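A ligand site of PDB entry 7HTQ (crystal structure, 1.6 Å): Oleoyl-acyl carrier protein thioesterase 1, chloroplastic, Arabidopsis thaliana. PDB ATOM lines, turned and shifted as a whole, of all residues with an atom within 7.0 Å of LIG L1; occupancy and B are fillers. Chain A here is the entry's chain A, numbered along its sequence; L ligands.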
ATOM      1  N   ALA A  71     -13.823  14.586  11.269  1.00  0.00           N
ATOM      2  CA  ALA A  71     -13.117  14.243  10.036  1.00  0.00           C
ATOM      3  C   ALA A  71     -13.725  12.956   9.412  1.00  0.00           C
ATOM      4  O   ALA A  71     -13.747  12.816   8.192  1.00  0.00           O
ATOM      5  CB  ALA A  71     -11.649  14.035  10.316  1.00  0.00           C
ATOM      6  N   ARG A  72     -14.211  12.036  10.237  1.00  0.00           N
ATOM      7  CA  ARG A  72     -14.827  10.804   9.760  1.00  0.00           C
ATOM      8  C   ARG A  72     -15.846  10.294  10.754  1.00  0.00           C
ATOM      9  O   ARG A  72     -15.641  10.439  11.969  1.00  0.00           O
ATOM     10  CB  ARG A  72     -13.768   9.702   9.511  1.00  0.00           C
ATOM     11  CG  ARG A  72     -14.354   8.306   9.245  1.00  0.00           C
ATOM     12  CD  ARG A  72     -13.301   7.291   8.897  1.00  0.00           C
ATOM     13  NE  ARG A  72     -12.834   7.520   7.549  1.00  0.00           N
ATOM     14  CZ  ARG A  72     -12.080   6.664   6.844  1.00  0.00           C
ATOM     15  NH1 ARG A  72     -11.674   5.519   7.390  1.00  0.00           N
ATOM     16  NH2 ARG A  72     -11.716   6.964   5.606  1.00  0.00           N
ATOM     17  N   GLN A  94     -11.230   9.274  23.437  1.00  0.00           N
ATOM     18  CA  GLN A  94      -9.819   8.960  23.696  1.00  0.00           C
ATOM     19  C   GLN A  94      -8.937   9.880  22.867  1.00  0.00           C
ATOM     20  O   GLN A  94      -9.256  10.161  21.704  1.00  0.00           O
ATOM     21  CB  GLN A  94      -9.462   7.503  23.305  1.00  0.00           C
ATOM     22  CG  GLN A  94     -10.035   6.371  24.158  1.00  0.00           C
ATOM     23  CD  GLN A  94      -9.017   5.251  24.313  1.00  0.00           C
ATOM     24  OE1 GLN A  94      -8.933   4.321  23.469  1.00  0.00           O
ATOM     25  NE2 GLN A  94      -8.215   5.365  25.394  1.00  0.00           N
ATOM     26  N   SER A  95      -7.771  10.295  23.427  1.00  0.00           N
ATOM     27  CA  SER A  95      -6.785  11.062  22.662  1.00  0.00           C
ATOM     28  C   SER A  95      -6.070  10.072  21.731  1.00  0.00           C
ATOM     29  O   SER A  95      -5.887   8.889  22.063  1.00  0.00           O
ATOM     30  CB  SER A  95      -5.737  11.664  23.589  1.00  0.00           C
ATOM     31  OG  SER A  95      -5.956  13.026  23.904  1.00  0.00           O
ATOM     32  N   GLU A  96      -5.708  10.534  20.542  1.00  0.00           N
ATOM     33  CA  GLU A  96      -4.948   9.717  19.610  1.00  0.00           C
ATOM     34  C   GLU A  96      -3.670  10.512  19.321  1.00  0.00           C
ATOM     35  O   GLU A  96      -3.418  10.887  18.193  1.00  0.00           O
ATOM     36  CB  GLU A  96      -5.754   9.358  18.360  1.00  0.00           C
ATOM     37  CG  GLU A  96      -6.931   8.448  18.689  1.00  0.00           C
ATOM     38  CD  GLU A  96      -7.549   7.726  17.508  1.00  0.00           C
ATOM     39  OE1 GLU A  96      -7.668   8.340  16.418  1.00  0.00           O
ATOM     40  OE2 GLU A  96      -7.930   6.546  17.666  1.00  0.00           O
ATOM     41  N   ILE A  99      -2.528  13.943  16.801  1.00  0.00           N
ATOM     42  CA  ILE A  99      -3.295  14.002  15.566  1.00  0.00           C
ATOM     43  C   ILE A  99      -4.709  14.526  15.856  1.00  0.00           C
ATOM     44  O   ILE A  99      -5.240  15.349  15.114  1.00  0.00           O
ATOM     45  CB  ILE A  99      -3.394  12.618  14.858  1.00  0.00           C
ATOM     46  CG1 ILE A  99      -2.090  11.822  14.890  1.00  0.00           C
ATOM     47  CG2 ILE A  99      -3.899  12.788  13.445  1.00  0.00           C
ATOM     48  CD1 ILE A  99      -2.305  10.332  14.485  1.00  0.00           C
ATOM     49  N   GLY A 100      -5.329  13.997  16.907  1.00  0.00           N
ATOM     50  CA  GLY A 100      -6.694  14.373  17.241  1.00  0.00           C
ATOM     51  C   GLY A 100      -7.305  13.491  18.305  1.00  0.00           C
ATOM     52  O   GLY A 100      -6.589  12.945  19.167  1.00  0.00           O
ATOM     53  N   THR A 101      -8.622  13.413  18.305  1.00  0.00           N
ATOM     54  CA  THR A 101      -9.341  12.635  19.302  1.00  0.00           C
ATOM     55  C   THR A 101     -10.328  11.691  18.602  1.00  0.00           C
ATOM     56  O   THR A 101     -10.670  11.884  17.436  1.00  0.00           O
ATOM     57  CB  THR A 101     -10.059  13.543  20.332  1.00  0.00           C
ATOM     58  OG1 THR A 101     -10.904  14.468  19.655  1.00  0.00           O
ATOM     59  CG2 THR A 101      -9.083  14.315  21.212  1.00  0.00           C
ATOM     60  N   ARG A 102     -10.804  10.694  19.333  1.00  0.00           N
ATOM     61  CA  ARG A 102     -11.777   9.756  18.803  1.00  0.00           C
ATOM     62  C   ARG A 102     -12.962   9.688  19.780  1.00  0.00           C
ATOM     63  O   ARG A 102     -12.749   9.829  20.972  1.00  0.00           O
ATOM     64  CB  ARG A 102     -11.108   8.362  18.736  1.00  0.00           C
ATOM     65  CG  ARG A 102     -11.873   7.335  17.943  1.00  0.00           C
ATOM     66  CD  ARG A 102     -11.175   5.983  17.984  1.00  0.00           C
ATOM     67  NE  ARG A 102     -11.564   5.273  19.189  1.00  0.00           N
ATOM     68  CZ  ARG A 102     -10.777   5.058  20.235  1.00  0.00           C
ATOM     69  NH1 ARG A 102     -11.247   4.444  21.313  1.00  0.00           N
ATOM     70  NH2 ARG A 102      -9.518   5.479  20.228  1.00  0.00           N
ATOM     71  N   SER A 121     -15.746   7.768  15.546  1.00  0.00           N
ATOM     72  CA  SER A 121     -15.523   8.994  14.804  1.00  0.00           C
ATOM     73  C   SER A 121     -14.156   9.566  15.096  1.00  0.00           C
ATOM     74  O   SER A 121     -13.684   9.472  16.245  1.00  0.00           O
ATOM     75  CB  SER A 121     -16.620   9.993  15.125  1.00  0.00           C
ATOM     76  OG  SER A 121     -16.609  10.264  16.518  1.00  0.00           O
ATOM     77  N   LYS A 122     -13.554  10.209  14.082  1.00  0.00           N
ATOM     78  CA  LYS A 122     -12.252  10.872  14.202  1.00  0.00           C
ATOM     79  C   LYS A 122     -12.494  12.378  14.203  1.00  0.00           C
ATOM     80  O   LYS A 122     -13.271  12.868  13.367  1.00  0.00           O
ATOM     81  CB  LYS A 122     -11.359  10.534  13.017  1.00  0.00           C
ATOM     82  CG  LYS A 122     -11.125   9.060  12.808  1.00  0.00           C
ATOM     83  CD  LYS A 122     -10.245   8.496  13.910  1.00  0.00           C
ATOM     84  CE  LYS A 122      -9.675   7.165  13.536  1.00  0.00           C
ATOM     85  NZ  LYS A 122      -8.825   6.611  14.631  1.00  0.00           N
ATOM     86  N   TRP A 123     -11.864  13.087  15.132  1.00  0.00           N
ATOM     87  CA  TRP A 123     -11.980  14.517  15.271  1.00  0.00           C
ATOM     88  C   TRP A 123     -10.590  15.175  15.204  1.00  0.00           C
ATOM     89  O   TRP A 123      -9.618  14.638  15.731  1.00  0.00           O
ATOM     90  CB  TRP A 123     -12.638  14.852  16.628  1.00  0.00           C
ATOM     91  CG  TRP A 123     -14.032  14.304  16.786  1.00  0.00           C
ATOM     92  CD1 TRP A 123     -14.384  13.001  16.995  1.00  0.00           C
ATOM     93  CD2 TRP A 123     -15.250  15.062  16.834  1.00  0.00           C
ATOM     94  NE1 TRP A 123     -15.755  12.893  17.099  1.00  0.00           N
ATOM     95  CE2 TRP A 123     -16.305  14.143  17.024  1.00  0.00           C
ATOM     96  CE3 TRP A 123     -15.553  16.423  16.686  1.00  0.00           C
ATOM     97  CZ2 TRP A 123     -17.638  14.547  17.086  1.00  0.00           C
ATOM     98  CZ3 TRP A 123     -16.878  16.822  16.746  1.00  0.00           C
ATOM     99  CH2 TRP A 123     -17.897  15.904  16.971  1.00  0.00           C
ATOM    100  N   VAL A 124     -10.496  16.339  14.553  1.00  0.00           N
ATOM    101  CA  VAL A 124      -9.262  17.116  14.426  1.00  0.00           C
ATOM    102  C   VAL A 124      -9.488  18.491  15.068  1.00  0.00           C
ATOM    103  O   VAL A 124     -10.631  18.950  15.180  1.00  0.00           O
ATOM    104  CB  VAL A 124      -8.783  17.294  12.962  1.00  0.00           C
ATOM    105  CG1 VAL A 124      -8.339  15.965  12.355  1.00  0.00           C
ATOM    106  CG2 VAL A 124      -9.848  17.951  12.104  1.00  0.00           C
ATOM    107  N   LEU A 133      -5.966  23.355  10.212  1.00  0.00           N
ATOM    108  CA  LEU A 133      -5.842  22.287  11.210  1.00  0.00           C
ATOM    109  C   LEU A 133      -4.580  22.467  12.024  1.00  0.00           C
ATOM    110  O   LEU A 133      -3.596  23.023  11.540  1.00  0.00           O
ATOM    111  CB  LEU A 133      -5.786  20.917  10.511  1.00  0.00           C
ATOM    112  CG  LEU A 133      -6.997  20.534   9.663  1.00  0.00           C
ATOM    113  CD1 LEU A 133      -6.891  19.106   9.183  1.00  0.00           C
ATOM    114  CD2 LEU A 133      -8.309  20.700  10.450  1.00  0.00           C
ATOM    115  N   LYS A 166      -8.842   3.668   3.875  1.00  0.00           N
ATOM    116  CA  LYS A 166      -8.788   4.845   3.020  1.00  0.00           C
ATOM    117  C   LYS A 166      -9.958   4.734   2.000  1.00  0.00           C
ATOM    118  O   LYS A 166     -10.255   3.632   1.555  1.00  0.00           O
ATOM    119  CB  LYS A 166      -7.445   4.797   2.277  1.00  0.00           C
ATOM    120  CG  LYS A 166      -7.172   5.968   1.356  1.00  0.00           C
ATOM    121  CD  LYS A 166      -6.518   7.110   2.123  1.00  0.00           C
ATOM    122  CE  LYS A 166      -5.464   7.818   1.308  1.00  0.00           C
ATOM    123  NZ  LYS A 166      -4.149   7.126   1.385  1.00  0.00           N
ATOM    124  N   TYR A 224     -15.370  13.790   6.011  1.00  0.00           N
ATOM    125  CA  TYR A 224     -15.822  15.181   5.945  1.00  0.00           C
ATOM    126  C   TYR A 224     -14.573  15.980   5.518  1.00  0.00           C
ATOM    127  O   TYR A 224     -13.587  16.029   6.267  1.00  0.00           O
ATOM    128  CB  TYR A 224     -16.349  15.658   7.322  1.00  0.00           C
ATOM    129  CG  TYR A 224     -17.662  15.020   7.737  1.00  0.00           C
ATOM    130  CD1 TYR A 224     -17.705  13.732   8.246  1.00  0.00           C
ATOM    131  CD2 TYR A 224     -18.860  15.720   7.670  1.00  0.00           C
ATOM    132  CE1 TYR A 224     -18.910  13.133   8.628  1.00  0.00           C
ATOM    133  CE2 TYR A 224     -20.072  15.150   8.054  1.00  0.00           C
ATOM    134  CZ  TYR A 224     -20.091  13.846   8.530  1.00  0.00           C
ATOM    135  OH  TYR A 224     -21.294  13.272   8.913  1.00  0.00           O
HETATM  136  N1  LIG L   1      -8.133  11.183  15.563  1.00  0.00           N
HETATM  137  C1  LIG L   1      -6.058  11.380  10.252  1.00  0.00           C
HETATM  138  C2  LIG L   1      -6.732  11.339  11.603  1.00  0.00           C
HETATM  139  C3  LIG L   1      -7.541  12.347  12.121  1.00  0.00           C
HETATM  140  C4  LIG L   1      -8.037  12.286  13.411  1.00  0.00           C
HETATM  141  C5  LIG L   1      -7.691  11.228  14.260  1.00  0.00           C
HETATM  142  C6  LIG L   1      -6.355  10.315  12.474  1.00  0.00           C
HETATM  143  N2  LIG L   1      -6.561  12.112   9.240  1.00  0.00           N
HETATM  144  C7  LIG L   1      -7.996  14.117   8.929  1.00  0.00           C
HETATM  145  O1  LIG L   1      -4.977  10.802  10.136  1.00  0.00           O
HETATM  146  C8  LIG L   1      -7.936  12.641   9.219  1.00  0.00           C
HETATM  147  C9  LIG L   1      -5.756  12.387   8.039  1.00  0.00           C
HETATM  148  C10 LIG L   1      -5.670  11.211   7.102  1.00  0.00           C
HETATM  149  C11 LIG L   1      -6.797  10.270  13.777  1.00  0.00           C
HETATM  150  N1  LG2 L   2     -11.332  13.719   6.337  1.00  0.00           N
HETATM  151  C1  LG2 L   2      -8.567   8.791   5.862  1.00  0.00           C
HETATM  152  C2  LG2 L   2      -9.274  10.100   6.038  1.00  0.00           C
HETATM  153  C3  LG2 L   2     -10.397  10.212   6.852  1.00  0.00           C
HETATM  154  C4  LG2 L   2     -11.064  11.412   6.949  1.00  0.00           C
HETATM  155  C5  LG2 L   2     -10.668  12.517   6.209  1.00  0.00           C
HETATM  156  C6  LG2 L   2      -8.882  11.198   5.279  1.00  0.00           C
HETATM  157  N2  LG2 L   2      -8.331   7.995   6.924  1.00  0.00           N
HETATM  158  C7  LG2 L   2      -9.207   7.735   9.253  1.00  0.00           C
HETATM  159  O1  LG2 L   2      -8.262   8.447   4.723  1.00  0.00           O
HETATM  160  C8  LG2 L   2      -8.309   8.503   8.312  1.00  0.00           C
HETATM  161  C9  LG2 L   2      -7.973   6.581   6.737  1.00  0.00           C
HETATM  162  C10 LG2 L   2      -6.496   6.386   6.503  1.00  0.00           C
HETATM  163  C11 LG2 L   2      -9.560  12.399   5.368  1.00  0.00           C
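Merely in contact with LIG L1: Ala 71 (3.9 Å), Ile 99 (3.6 Å), Gly 100 (3.7 Å), Lys 122 (3.8 Å), Trp 123 (3.7 Å) and Val 124 (3.7 Å). Eight residues have an atom within 4 Å of LIG L1: Ala 71, Glu 96, Ile 99, Gly 100, Thr 101, Lys 122, Trp 123 and Val 124. The nearest printed residue that does not touch LIG L1 is Arg 102 (4.6 Å).
The side-chain carboxylate (OE1) of Glu 96 lies within salt-bridge range of the side-chain amino group (NZ) of Lys 122, at 2.7 Å. NH2 of Arg 102 is in salt-bridge range of OE2 of Glu 96 (3.2 Å). The backbone carbonyl oxygen (O) of Thr 101 lies within hydrogen-bond range of the backbone NH (N) of Trp 123 (2.9 Å). NE1 of Trp 123 is in hydrogen-bond range of OG of Ser 121 (2.8 Å). N of Ala 71 is in hydrogen-bond range of O of Lys 122, at 2.8 Å. The backbone NH (N) of Lys 122 is in hydrogen-bond range of the backbone carbonyl oxygen (O) of Arg 72, at 3.0 Å. O of Ala 71 is in hydrogen-bond range of N of Tyr 224 (2.9 Å).
N1 of LIG L1 is in hydrogen-bond range of OE1 of Glu 96 (3.0 Å). A nitrogen (N1) of LIG L1 is in hydrogen-bond range of the backbone carbonyl oxygen of Thr 101 (3.2 Å). O of Ala 71 lies within hydrogen-bond range of N1 of LG2 L2, at 3.2 Å. The backbone carbonyl oxygen of Tyr 224 lies within hydrogen-bond range of a nitrogen (N1) of LG2 L2.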
